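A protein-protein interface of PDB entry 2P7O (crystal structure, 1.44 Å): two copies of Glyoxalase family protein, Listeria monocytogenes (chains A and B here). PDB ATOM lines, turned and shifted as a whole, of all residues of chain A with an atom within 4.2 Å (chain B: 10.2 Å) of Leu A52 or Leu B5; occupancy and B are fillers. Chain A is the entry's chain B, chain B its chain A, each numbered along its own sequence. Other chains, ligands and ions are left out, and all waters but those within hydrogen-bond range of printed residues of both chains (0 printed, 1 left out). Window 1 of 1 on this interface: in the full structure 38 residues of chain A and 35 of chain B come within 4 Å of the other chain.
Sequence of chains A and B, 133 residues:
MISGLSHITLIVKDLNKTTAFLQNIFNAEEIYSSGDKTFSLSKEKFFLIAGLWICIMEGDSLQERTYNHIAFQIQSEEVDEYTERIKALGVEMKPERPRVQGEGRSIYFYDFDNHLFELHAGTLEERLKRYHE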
ATOM      1  N   LEU A   5     -18.656  26.283 -30.605  1.00  0.00           N
ATOM      2  CA  LEU A   5     -20.032  26.277 -30.139  1.00  0.00           C
ATOM      3  C   LEU A   5     -20.381  27.625 -29.518  1.00  0.00           C
ATOM      4  O   LEU A   5     -19.619  28.134 -28.683  1.00  0.00           O
ATOM      5  CB  LEU A   5     -20.182  25.174 -29.051  1.00  0.00           C
ATOM      6  CG  LEU A   5     -21.596  25.112 -28.477  1.00  0.00           C
ATOM      7  CD1 LEU A   5     -22.531  24.561 -29.585  1.00  0.00           C
ATOM      8  CD2 LEU A   5     -21.618  24.245 -27.224  1.00  0.00           C
ATOM      9  N   ILE A   8     -26.139  26.353 -26.205  1.00  0.00           N
ATOM     10  CA  ILE A   8     -27.320  25.514 -26.436  1.00  0.00           C
ATOM     11  C   ILE A   8     -28.486  26.151 -25.705  1.00  0.00           C
ATOM     12  O   ILE A   8     -28.238  26.601 -24.555  1.00  0.00           O
ATOM     13  CB  ILE A   8     -27.022  24.104 -25.887  1.00  0.00           C
ATOM     14  CG1 ILE A   8     -25.892  23.504 -26.768  1.00  0.00           C
ATOM     15  CG2 ILE A   8     -28.271  23.266 -25.888  1.00  0.00           C
ATOM     16  CD1 ILE A   8     -25.341  22.203 -26.131  1.00  0.00           C
ATOM     17  N   PHE A  47     -26.333  29.842 -17.991  1.00  0.00           N
ATOM     18  CA  PHE A  47     -25.384  29.200 -17.089  1.00  0.00           C
ATOM     19  C   PHE A  47     -24.136  28.817 -17.878  1.00  0.00           C
ATOM     20  O   PHE A  47     -24.191  28.576 -19.085  1.00  0.00           O
ATOM     21  CB  PHE A  47     -25.948  27.904 -16.523  1.00  0.00           C
ATOM     22  CG  PHE A  47     -27.166  27.994 -15.638  1.00  0.00           C
ATOM     23  CD1 PHE A  47     -28.412  28.107 -16.238  1.00  0.00           C
ATOM     24  CD2 PHE A  47     -27.086  27.988 -14.237  1.00  0.00           C
ATOM     25  CE1 PHE A  47     -29.578  28.282 -15.512  1.00  0.00           C
ATOM     26  CE2 PHE A  47     -28.262  28.072 -13.506  1.00  0.00           C
ATOM     27  CZ  PHE A  47     -29.507  28.174 -14.112  1.00  0.00           C
ATOM     28  N   LEU A  48     -23.058  28.627 -17.137  1.00  0.00           N
ATOM     29  CA  LEU A  48     -21.877  27.976 -17.716  1.00  0.00           C
ATOM     30  C   LEU A  48     -21.714  26.632 -17.000  1.00  0.00           C
ATOM     31  O   LEU A  48     -21.817  26.547 -15.779  1.00  0.00           O
ATOM     32  CB  LEU A  48     -20.555  28.727 -17.476  1.00  0.00           C
ATOM     33  CG  LEU A  48     -20.220  29.755 -18.557  1.00  0.00           C
ATOM     34  CD1 LEU A  48     -19.199  30.757 -18.021  1.00  0.00           C
ATOM     35  CD2 LEU A  48     -19.671  29.020 -19.769  1.00  0.00           C
ATOM     36  N   ILE A  49     -21.523  25.611 -17.802  1.00  0.00           N
ATOM     37  CA  ILE A  49     -21.149  24.285 -17.289  1.00  0.00           C
ATOM     38  C   ILE A  49     -19.887  23.895 -18.060  1.00  0.00           C
ATOM     39  O   ILE A  49     -20.046  23.707 -19.254  1.00  0.00           O
ATOM     40  CB  ILE A  49     -22.200  23.199 -17.549  1.00  0.00           C
ATOM     41  CG1 ILE A  49     -23.495  23.476 -16.787  1.00  0.00           C
ATOM     42  CG2 ILE A  49     -21.645  21.831 -17.168  1.00  0.00           C
ATOM     43  CD1 ILE A  49     -24.600  22.533 -17.062  1.00  0.00           C
ATOM     44  N   ALA A  50     -18.739  23.880 -17.423  1.00  0.00           N
ATOM     45  CA  ALA A  50     -17.529  23.371 -18.101  1.00  0.00           C
ATOM     46  C   ALA A  50     -17.272  23.939 -19.482  1.00  0.00           C
ATOM     47  O   ALA A  50     -16.961  23.310 -20.495  1.00  0.00           O
ATOM     48  CB  ALA A  50     -17.708  21.863 -18.144  1.00  0.00           C
ATOM     49  N   GLY A  51     -17.381  25.282 -19.547  1.00  0.00           N
ATOM     50  CA  GLY A  51     -17.044  25.938 -20.825  1.00  0.00           C
ATOM     51  C   GLY A  51     -18.190  26.078 -21.798  1.00  0.00           C
ATOM     52  O   GLY A  51     -18.056  26.728 -22.864  1.00  0.00           O
ATOM     53  N   LEU A  52     -19.340  25.507 -21.442  1.00  0.00           N
ATOM     54  CA  LEU A  52     -20.497  25.580 -22.339  1.00  0.00           C
ATOM     55  C   LEU A  52     -21.562  26.536 -21.818  1.00  0.00           C
ATOM     56  O   LEU A  52     -22.031  26.424 -20.681  1.00  0.00           O
ATOM     57  CB  LEU A  52     -21.027  24.151 -22.556  1.00  0.00           C
ATOM     58  CG  LEU A  52     -22.295  23.955 -23.378  1.00  0.00           C
ATOM     59  CD1 LEU A  52     -22.192  22.765 -24.332  1.00  0.00           C
ATOM     60  CD2 LEU A  52     -23.494  23.774 -22.443  1.00  0.00           C
ATOM     61  N   TRP A  53     -21.958  27.499 -22.660  1.00  0.00           N
ATOM     62  CA  TRP A  53     -23.040  28.417 -22.294  1.00  0.00           C
ATOM     63  C   TRP A  53     -24.376  27.754 -22.619  1.00  0.00           C
ATOM     64  O   TRP A  53     -24.628  27.379 -23.771  1.00  0.00           O
ATOM     65  CB  TRP A  53     -22.878  29.763 -23.010  1.00  0.00           C
ATOM     66  CG  TRP A  53     -21.543  30.435 -22.821  1.00  0.00           C
ATOM     67  CD1 TRP A  53     -20.400  30.117 -23.523  1.00  0.00           C
ATOM     68  CD2 TRP A  53     -21.166  31.511 -21.941  1.00  0.00           C
ATOM     69  NE1 TRP A  53     -19.353  30.921 -23.130  1.00  0.00           N
ATOM     70  CE2 TRP A  53     -19.813  31.787 -22.155  1.00  0.00           C
ATOM     71  CE3 TRP A  53     -21.853  32.270 -21.000  1.00  0.00           C
ATOM     72  CZ2 TRP A  53     -19.116  32.773 -21.468  1.00  0.00           C
ATOM     73  CZ3 TRP A  53     -21.165  33.266 -20.321  1.00  0.00           C
ATOM     74  CH2 TRP A  53     -19.806  33.527 -20.563  1.00  0.00           C
ATOM     75  N   ILE A  54     -25.182  27.561 -21.549  1.00  0.00           N
ATOM     76  CA  ILE A  54     -26.526  26.996 -21.710  1.00  0.00           C
ATOM     77  C   ILE A  54     -27.630  27.972 -21.347  1.00  0.00           C
ATOM     78  O   ILE A  54     -27.684  28.526 -20.237  1.00  0.00           O
ATOM     79  CB  ILE A  54     -26.673  25.710 -20.886  1.00  0.00           C
ATOM     80  CG1 ILE A  54     -28.035  25.041 -21.115  1.00  0.00           C
ATOM     81  CG2 ILE A  54     -26.460  25.900 -19.396  1.00  0.00           C
ATOM     82  CD1 ILE A  54     -27.986  23.538 -20.834  1.00  0.00           C
ATOM     83  N   ILE A  70     -27.545  15.454 -24.863  1.00  0.00           N
ATOM     84  CA  ILE A  70     -26.288  16.113 -24.525  1.00  0.00           C
ATOM     85  C   ILE A  70     -25.515  15.243 -23.514  1.00  0.00           C
ATOM     86  O   ILE A  70     -26.139  14.958 -22.480  1.00  0.00           O
ATOM     87  CB  ILE A  70     -26.572  17.483 -23.840  1.00  0.00           C
ATOM     88  CG1 ILE A  70     -27.376  18.342 -24.832  1.00  0.00           C
ATOM     89  CG2 ILE A  70     -25.277  18.190 -23.494  1.00  0.00           C
ATOM     90  CD1 ILE A  70     -26.602  18.346 -26.146  1.00  0.00           C
ATOM     91  N   ALA A  71     -24.267  14.890 -23.806  1.00  0.00           N
ATOM     92  CA  ALA A  71     -23.404  14.162 -22.863  1.00  0.00           C
ATOM     93  C   ALA A  71     -22.279  15.109 -22.398  1.00  0.00           C
ATOM     94  O   ALA A  71     -21.547  15.637 -23.244  1.00  0.00           O
ATOM     95  CB  ALA A  71     -22.721  12.992 -23.551  1.00  0.00           C
ATOM     96  N   PHE A  72     -22.115  15.125 -21.085  1.00  0.00           N
ATOM     97  CA  PHE A  72     -21.038  15.804 -20.383  1.00  0.00           C
ATOM     98  C   PHE A  72     -19.994  14.784 -19.907  1.00  0.00           C
ATOM     99  O   PHE A  72     -20.358  13.681 -19.544  1.00  0.00           O
ATOM    100  CB  PHE A  72     -21.577  16.597 -19.178  1.00  0.00           C
ATOM    101  CG  PHE A  72     -22.342  17.843 -19.619  1.00  0.00           C
ATOM    102  CD1 PHE A  72     -23.730  17.779 -19.671  1.00  0.00           C
ATOM    103  CD2 PHE A  72     -21.719  19.017 -19.969  1.00  0.00           C
ATOM    104  CE1 PHE A  72     -24.459  18.901 -20.068  1.00  0.00           C
ATOM    105  CE2 PHE A  72     -22.432  20.131 -20.374  1.00  0.00           C
ATOM    106  CZ  PHE A  72     -23.823  20.098 -20.396  1.00  0.00           C
ATOM    107  N   MET B   1     -16.985  15.022 -12.901  1.00  0.00           N
ATOM    108  CA  MET B   1     -15.868  15.939 -13.213  1.00  0.00           C
ATOM    109  C   MET B   1     -16.332  17.367 -13.116  1.00  0.00           C
ATOM    110  O   MET B   1     -16.075  17.888 -11.973  1.00  0.00           O
ATOM    111  CB  MET B   1     -15.002  15.255 -14.187  1.00  0.00           C
ATOM    112  CG  MET B   1     -13.962  15.748 -15.136  1.00  0.00           C
ATOM    113  SD  MET B   1     -12.308  15.872 -14.416  1.00  0.00           S
ATOM    114  CE  MET B   1     -12.083  17.655 -14.472  1.00  0.00           C
ATOM    115  N   ILE B   2     -17.113  18.094 -13.876  1.00  0.00           N
ATOM    116  CA  ILE B   2     -17.525  18.044 -15.249  1.00  0.00           C
ATOM    117  C   ILE B   2     -16.329  18.591 -16.042  1.00  0.00           C
ATOM    118  O   ILE B   2     -16.042  19.770 -15.794  1.00  0.00           O
ATOM    119  CB  ILE B   2     -18.740  18.926 -15.578  1.00  0.00           C
ATOM    120  CG1 ILE B   2     -19.958  18.758 -14.667  1.00  0.00           C
ATOM    121  CG2 ILE B   2     -19.091  18.748 -17.062  1.00  0.00           C
ATOM    122  CD1 ILE B   2     -20.834  17.580 -15.006  1.00  0.00           C
ATOM    123  N   SER B   3     -15.623  17.792 -16.809  1.00  0.00           N
ATOM    124  CA  SER B   3     -14.473  18.346 -17.533  1.00  0.00           C
ATOM    125  C   SER B   3     -14.908  19.226 -18.688  1.00  0.00           C
ATOM    126  O   SER B   3     -14.253  20.198 -19.119  1.00  0.00           O
ATOM    127  CB  SER B   3     -13.594  17.211 -18.060  1.00  0.00           C
ATOM    128  N   GLY B   4     -15.979  18.781 -19.327  1.00  0.00           N
ATOM    129  CA  GLY B   4     -16.412  19.497 -20.534  1.00  0.00           C
ATOM    130  C   GLY B   4     -17.533  18.700 -21.186  1.00  0.00           C
ATOM    131  O   GLY B   4     -18.105  17.803 -20.595  1.00  0.00           O
ATOM    132  N   LEU B   5     -17.869  19.118 -22.396  1.00  0.00           N
ATOM    133  CA  LEU B   5     -18.796  18.423 -23.253  1.00  0.00           C
ATOM    134  C   LEU B   5     -18.075  17.156 -23.718  1.00  0.00           C
ATOM    135  O   LEU B   5     -16.896  17.179 -24.129  1.00  0.00           O
ATOM    136  CB  LEU B   5     -19.180  19.337 -24.434  1.00  0.00           C
ATOM    137  CG  LEU B   5     -20.514  19.086 -25.107  1.00  0.00           C
ATOM    138  CD1 LEU B   5     -21.649  19.210 -24.090  1.00  0.00           C
ATOM    139  CD2 LEU B   5     -20.794  20.093 -26.216  1.00  0.00           C
ATOM    140  N   SER B   6     -18.765  16.039 -23.645  1.00  0.00           N
ATOM    141  CA  SER B   6     -18.389  14.780 -24.255  1.00  0.00           C
ATOM    142  C   SER B   6     -18.837  14.746 -25.727  1.00  0.00           C
ATOM    143  O   SER B   6     -17.981  14.582 -26.601  1.00  0.00           O
ATOM    144  CB  SER B   6     -19.068  13.570 -23.553  1.00  0.00           C
ATOM    145  OG  SER B   6     -18.679  12.386 -24.237  1.00  0.00           O
ATOM    146  N   HIS B   7     -20.139  14.903 -25.940  1.00  0.00           N
ATOM    147  CA  HIS B   7     -20.637  14.789 -27.333  1.00  0.00           C
ATOM    148  C   HIS B   7     -22.094  15.220 -27.306  1.00  0.00           C
ATOM    149  O   HIS B   7     -22.697  15.297 -26.233  1.00  0.00           O
ATOM    150  CB  HIS B   7     -20.495  13.368 -27.903  1.00  0.00           C
ATOM    151  CG  HIS B   7     -21.198  12.273 -27.174  1.00  0.00           C
ATOM    152  ND1 HIS B   7     -20.595  11.709 -26.027  1.00  0.00           N
ATOM    153  CD2 HIS B   7     -22.365  11.613 -27.315  1.00  0.00           C
ATOM    154  CE1 HIS B   7     -21.369  10.745 -25.532  1.00  0.00           C
ATOM    155  NE2 HIS B   7     -22.451  10.668 -26.291  1.00  0.00           N
ATOM    156  N   ILE B   8     -22.656  15.388 -28.495  1.00  0.00           N
ATOM    157  CA  ILE B   8     -24.111  15.468 -28.615  1.00  0.00           C
ATOM    158  C   ILE B   8     -24.547  14.395 -29.603  1.00  0.00           C
ATOM    159  O   ILE B   8     -23.829  14.207 -30.596  1.00  0.00           O
ATOM    160  CB  ILE B   8     -24.430  16.856 -29.155  1.00  0.00           C
ATOM    161  CG1 ILE B   8     -24.021  17.967 -28.157  1.00  0.00           C
ATOM    162  CG2 ILE B   8     -25.894  16.989 -29.488  1.00  0.00           C
ATOM    163  CD1 ILE B   8     -24.250  19.355 -28.761  1.00  0.00           C
ATOM    164  N   THR B   9     -25.619  13.705 -29.346  1.00  0.00           N
ATOM    165  CA  THR B   9     -26.101  12.655 -30.240  1.00  0.00           C
ATOM    166  C   THR B   9     -27.479  13.078 -30.751  1.00  0.00           C
ATOM    167  O   THR B   9     -28.390  13.371 -29.958  1.00  0.00           O
ATOM    168  CB  THR B   9     -26.153  11.316 -29.464  1.00  0.00           C
ATOM    169  OG1 THR B   9     -24.778  10.900 -29.279  1.00  0.00           O
ATOM    170  CG2 THR B   9     -26.954  10.251 -30.205  1.00  0.00           C
ATOM    171  N   PHE B  46     -19.947   9.434 -36.500  1.00  0.00           N
ATOM    172  CA  PHE B  46     -19.457  10.577 -35.721  1.00  0.00           C
ATOM    173  C   PHE B  46     -18.846  11.627 -36.664  1.00  0.00           C
ATOM    174  O   PHE B  46     -18.177  11.303 -37.650  1.00  0.00           O
ATOM    175  CB  PHE B  46     -18.451  10.141 -34.658  1.00  0.00           C
ATOM    176  CG  PHE B  46     -19.007   9.861 -33.272  1.00  0.00           C
ATOM    177  CD1 PHE B  46     -18.945  10.819 -32.280  1.00  0.00           C
ATOM    178  CD2 PHE B  46     -19.564   8.608 -32.994  1.00  0.00           C
ATOM    179  CE1 PHE B  46     -19.427  10.551 -30.998  1.00  0.00           C
ATOM    180  CE2 PHE B  46     -20.041   8.343 -31.730  1.00  0.00           C
ATOM    181  CZ  PHE B  46     -19.994   9.329 -30.731  1.00  0.00           C
ATOM    182  N   LEU B  48     -16.957  15.824 -36.341  1.00  0.00           N
ATOM    183  CA  LEU B  48     -16.369  16.881 -35.572  1.00  0.00           C
ATOM    184  C   LEU B  48     -16.760  18.198 -36.262  1.00  0.00           C
ATOM    185  O   LEU B  48     -16.520  18.319 -37.481  1.00  0.00           O
ATOM    186  CB  LEU B  48     -14.828  16.887 -35.620  1.00  0.00           C
ATOM    187  CG  LEU B  48     -14.236  15.583 -35.085  1.00  0.00           C
ATOM    188  CD1 LEU B  48     -12.807  15.656 -34.593  1.00  0.00           C
ATOM    189  CD2 LEU B  48     -15.209  15.265 -33.975  1.00  0.00           C
ATOM    190  N   ILE B  49     -17.239  19.113 -35.444  1.00  0.00           N
ATOM    191  CA  ILE B  49     -17.586  20.475 -35.845  1.00  0.00           C
ATOM    192  C   ILE B  49     -16.980  21.435 -34.807  1.00  0.00           C
ATOM    193  O   ILE B  49     -17.503  21.568 -33.697  1.00  0.00           O
ATOM    194  CB  ILE B  49     -19.115  20.631 -35.886  1.00  0.00           C
ATOM    195  CG1 ILE B  49     -19.821  19.560 -36.738  1.00  0.00           C
ATOM    196  CG2 ILE B  49     -19.487  22.036 -36.393  1.00  0.00           C
ATOM    197  CD1 ILE B  49     -21.318  19.757 -36.727  1.00  0.00           C
ATOM    198  N   ALA B  50     -15.869  22.020 -35.252  1.00  0.00           N
ATOM    199  CA  ALA B  50     -15.186  23.043 -34.465  1.00  0.00           C
ATOM    200  C   ALA B  50     -14.988  22.546 -33.030  1.00  0.00           C
ATOM    201  O   ALA B  50     -15.249  23.242 -32.049  1.00  0.00           O
ATOM    202  CB  ALA B  50     -15.980  24.327 -34.497  1.00  0.00           C
ATOM    203  N   GLY B  51     -14.622  21.274 -32.962  1.00  0.00           N
ATOM    204  CA  GLY B  51     -14.226  20.704 -31.650  1.00  0.00           C
ATOM    205  C   GLY B  51     -15.357  19.934 -30.979  1.00  0.00           C
ATOM    206  O   GLY B  51     -15.182  19.201 -29.977  1.00  0.00           O
ATOM    207  N   LEU B  52     -16.572  20.156 -31.448  1.00  0.00           N
ATOM    208  CA  LEU B  52     -17.686  19.398 -30.866  1.00  0.00           C
ATOM    209  C   LEU B  52     -17.745  18.041 -31.589  1.00  0.00           C
ATOM    210  O   LEU B  52     -17.778  17.982 -32.830  1.00  0.00           O
ATOM    211  CB  LEU B  52     -19.010  20.143 -31.075  1.00  0.00           C
ATOM    212  CG  LEU B  52     -20.315  19.334 -30.934  1.00  0.00           C
ATOM    213  CD1 LEU B  52     -20.564  18.985 -29.473  1.00  0.00           C
ATOM    214  CD2 LEU B  52     -21.460  20.092 -31.584  1.00  0.00           C
ATOM    215  N   TRP B  53     -17.798  16.967 -30.815  1.00  0.00           N
ATOM    216  CA  TRP B  53     -18.049  15.616 -31.271  1.00  0.00           C
ATOM    217  C   TRP B  53     -19.545  15.362 -31.382  1.00  0.00           C
ATOM    218  O   TRP B  53     -20.262  15.318 -30.372  1.00  0.00           O
ATOM    219  CB  TRP B  53     -17.410  14.587 -30.306  1.00  0.00           C
ATOM    220  CG  TRP B  53     -15.904  14.630 -30.323  1.00  0.00           C
ATOM    221  CD1 TRP B  53     -15.138  15.500 -29.559  1.00  0.00           C
ATOM    222  CD2 TRP B  53     -14.969  13.801 -31.043  1.00  0.00           C
ATOM    223  NE1 TRP B  53     -13.805  15.250 -29.796  1.00  0.00           N
ATOM    224  CE2 TRP B  53     -13.682  14.226 -30.696  1.00  0.00           C
ATOM    225  CE3 TRP B  53     -15.110  12.719 -31.945  1.00  0.00           C
ATOM    226  CZ2 TRP B  53     -12.506  13.653 -31.219  1.00  0.00           C
ATOM    227  CZ3 TRP B  53     -13.959  12.156 -32.474  1.00  0.00           C
ATOM    228  CH2 TRP B  53     -12.684  12.620 -32.111  1.00  0.00           C
ATOM    229  N   ILE B  54     -19.985  15.200 -32.635  1.00  0.00           N
ATOM    230  CA  ILE B  54     -21.406  14.940 -32.809  1.00  0.00           C
ATOM    231  C   ILE B  54     -21.654  13.564 -33.402  1.00  0.00           C
ATOM    232  O   ILE B  54     -21.038  13.193 -34.418  1.00  0.00           O
ATOM    233  CB  ILE B  54     -22.087  16.081 -33.566  1.00  0.00           C
ATOM    234  CG1 ILE B  54     -23.605  15.848 -33.715  1.00  0.00           C
ATOM    235  CG2 ILE B  54     -21.431  16.413 -34.885  1.00  0.00           C
ATOM    236  CD1 ILE B  54     -24.454  17.110 -33.658  1.00  0.00           C
ATOM    237  N   CYS B  55     -22.517  12.801 -32.716  1.00  0.00           N
ATOM    238  CA  CYS B  55     -22.921  11.503 -33.273  1.00  0.00           C
ATOM    239  C   CYS B  55     -24.304  11.618 -33.869  1.00  0.00           C
ATOM    240  O   CYS B  55     -25.224  12.233 -33.244  1.00  0.00           O
ATOM    241  CB  CYS B  55     -22.967  10.493 -32.081  1.00  0.00           C
ATOM    242  SG  CYS B  55     -23.756   8.935 -32.496  1.00  0.00           S
ATOM    243  N   HIS B  69     -32.431  24.398 -29.250  1.00  0.00           N
ATOM    244  CA  HIS B  69     -31.556  24.460 -30.412  1.00  0.00           C
ATOM    245  C   HIS B  69     -30.093  24.490 -29.971  1.00  0.00           C
ATOM    246  O   HIS B  69     -29.742  24.999 -28.884  1.00  0.00           O
ATOM    247  CB  HIS B  69     -31.798  25.705 -31.258  1.00  0.00           C
ATOM    248  CG  HIS B  69     -31.668  27.046 -30.589  1.00  0.00           C
ATOM    249  ND1 HIS B  69     -32.694  27.613 -29.858  1.00  0.00           N
ATOM    250  CD2 HIS B  69     -30.663  27.956 -30.560  1.00  0.00           C
ATOM    251  CE1 HIS B  69     -32.297  28.823 -29.397  1.00  0.00           C
ATOM    252  NE2 HIS B  69     -31.058  29.040 -29.818  1.00  0.00           N
ATOM    253  N   ILE B  70     -29.284  24.077 -30.939  1.00  0.00           N
ATOM    254  CA  ILE B  70     -27.805  24.137 -30.793  1.00  0.00           C
ATOM    255  C   ILE B  70     -27.366  25.304 -31.664  1.00  0.00           C
ATOM    256  O   ILE B  70     -27.777  25.378 -32.816  1.00  0.00           O
ATOM    257  CB  ILE B  70     -27.175  22.836 -31.284  1.00  0.00           C
ATOM    258  CG1 ILE B  70     -27.679  21.613 -30.490  1.00  0.00           C
ATOM    259  CG2 ILE B  70     -25.646  22.935 -31.241  1.00  0.00           C
ATOM    260  CD1 ILE B  70     -27.367  20.287 -31.192  1.00  0.00           C
ATOM    261  N   ALA B  71     -26.527  26.158 -31.133  1.00  0.00           N
ATOM    262  CA  ALA B  71     -26.093  27.360 -31.884  1.00  0.00           C
ATOM    263  C   ALA B  71     -24.572  27.276 -32.055  1.00  0.00           C
ATOM    264  O   ALA B  71     -23.829  27.082 -31.064  1.00  0.00           O
ATOM    265  CB  ALA B  71     -26.472  28.596 -31.059  1.00  0.00           C
ATOM    266  N   PHE B  72     -24.055  27.433 -33.261  1.00  0.00           N
ATOM    267  CA  PHE B  72     -22.629  27.535 -33.510  1.00  0.00           C
ATOM    268  C   PHE B  72     -22.245  28.989 -33.813  1.00  0.00           C
ATOM    269  O   PHE B  72     -23.061  29.722 -34.348  1.00  0.00           O
ATOM    270  CB  PHE B  72     -22.233  26.702 -34.754  1.00  0.00           C
ATOM    271  CG  PHE B  72     -22.268  25.207 -34.415  1.00  0.00           C
ATOM    272  CD1 PHE B  72     -23.349  24.425 -34.773  1.00  0.00           C
ATOM    273  CD2 PHE B  72     -21.175  24.612 -33.808  1.00  0.00           C
ATOM    274  CE1 PHE B  72     -23.308  23.060 -34.509  1.00  0.00           C
ATOM    275  CE2 PHE B  72     -21.180  23.283 -33.438  1.00  0.00           C
ATOM    276  CZ  PHE B  72     -22.248  22.483 -33.823  1.00  0.00           C
ATOM    277  N   LEU B 124     -23.215  37.267 -27.470  1.00  0.00           N
ATOM    278  CA  LEU B 124     -24.032  36.183 -26.963  1.00  0.00           C
ATOM    279  C   LEU B 124     -25.325  36.658 -26.315  1.00  0.00           C
ATOM    280  O   LEU B 124     -25.263  37.351 -25.304  1.00  0.00           O
ATOM    281  CB  LEU B 124     -23.192  35.383 -25.929  1.00  0.00           C
ATOM    282  CG  LEU B 124     -23.877  34.130 -25.345  1.00  0.00           C
ATOM    283  CD1 LEU B 124     -24.119  33.147 -26.501  1.00  0.00           C
ATOM    284  CD2 LEU B 124     -23.068  33.414 -24.259  1.00  0.00           C
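N of Ile B8 sits at hydrogen-bond distance from O of Trp B53, 3.0 Å away. OG of Ser B6 is in hydrogen-bond range of ND1 of His B7 (2.7 Å). O of Ile B8 lies within hydrogen-bond range of N of Cys B55 (2.9 Å). O of Trp A53 is in hydrogen-bond range of N of Ile A8 (3.0 Å).
Leu A5 touches Ile B70, and with the chains exchanged Ile A70 touches Leu B5. Leu A5 touches Ala B71, and with the chains exchanged Ala A71 touches Leu B5. Leu A52 touches Leu B5, but with the chains exchanged Leu A5 does not touch Leu B52 (5.0 Å). Ile A70 touches Ile B8, but with the chains exchanged Ile A8 does not touch Ile B70 (4.5 Å). Of the 18 pairs that touch across the chains among the printed residues, 4 have their exchanged pair printed and touching as well.
Printed residues of chain B that touch a printed residue of chain A: Ile B2, Ser B3, Gly B4, Leu B5, Ser B6, His B7, Ile B8, His B69, Ile B70, Ala B71 and Leu B124. Hydrophobic or aromatic side chains of chain B that line the printed part of chain A: Ile B2, Leu B5, His B7, Ile B8, Ile B70 and Leu B124. Printed residues of chain A that touch a printed residue of chain B: Leu A5, Ile A8, Ala A50, Leu A52, Trp A53, Ile A70, Ala A71 and Phe A72. Among the printed residues, 18 pairs touch across the chains. Among the printed residues, no Asp or Glu carboxylate lies within 4 Å of a Lys or Arg side-chain nitrogen of the other chain.
N of Ser B6 lies within hydrogen-bond range of O of Ala A71, 2.8 Å away. The backbone carbonyl oxygen (O) of His B7 sits at hydrogen-bond distance from the backbone NH (N) of Ala A71 (2.9 Å).
Ala A50 touches just these residues of chain B: Ile B2, Ser B3 and Gly B4. Gly A51 touches none of the printed residues of chain B. Of chain B, only Leu B5 (3.6 Å) comes within 4 Å of Leu A52. Ile A54 touches none of the printed residues of chain B. Of the printed residues of chain B, Ala A71 touches Leu B5, Ser B6 and His B7. Of chain B, only Ile B2 (3.9 Å), Gly B4 (3.6 Å), Leu B5 (3.9 Å) and Ser B6 (3.95 Å) come within 4 Å of Phe A72. Printed residues of chain A within 4 Å of Ser B3: Ala A50. Leu B5 touches just these residues of chain A: Leu A52, Ile A70, Ala A71 and Phe A72. The nearest printed residue of chain A that does not touch Gly B4 is Ala A71 (4.9 Å).
Among the printed residues, merely in contact across the chains: Leu A5 with Ile B70, Leu A5 with Ala B71, Ile A8 with His B69, Ala A50 with Ile B2, Ala A50 with Ser B3, Ala A50 with Gly B4, Leu A52 with Leu B5, Trp A53 with Leu B124, Ile A70 with Leu B5, Ile A70 with His B7, Ile A70 with Ile B8, Ala A71 with Leu B5, Phe A72 with Ile B2, Phe A72 with Gly B4, Phe A72 with Leu B5 and Phe A72 with Ser B6.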
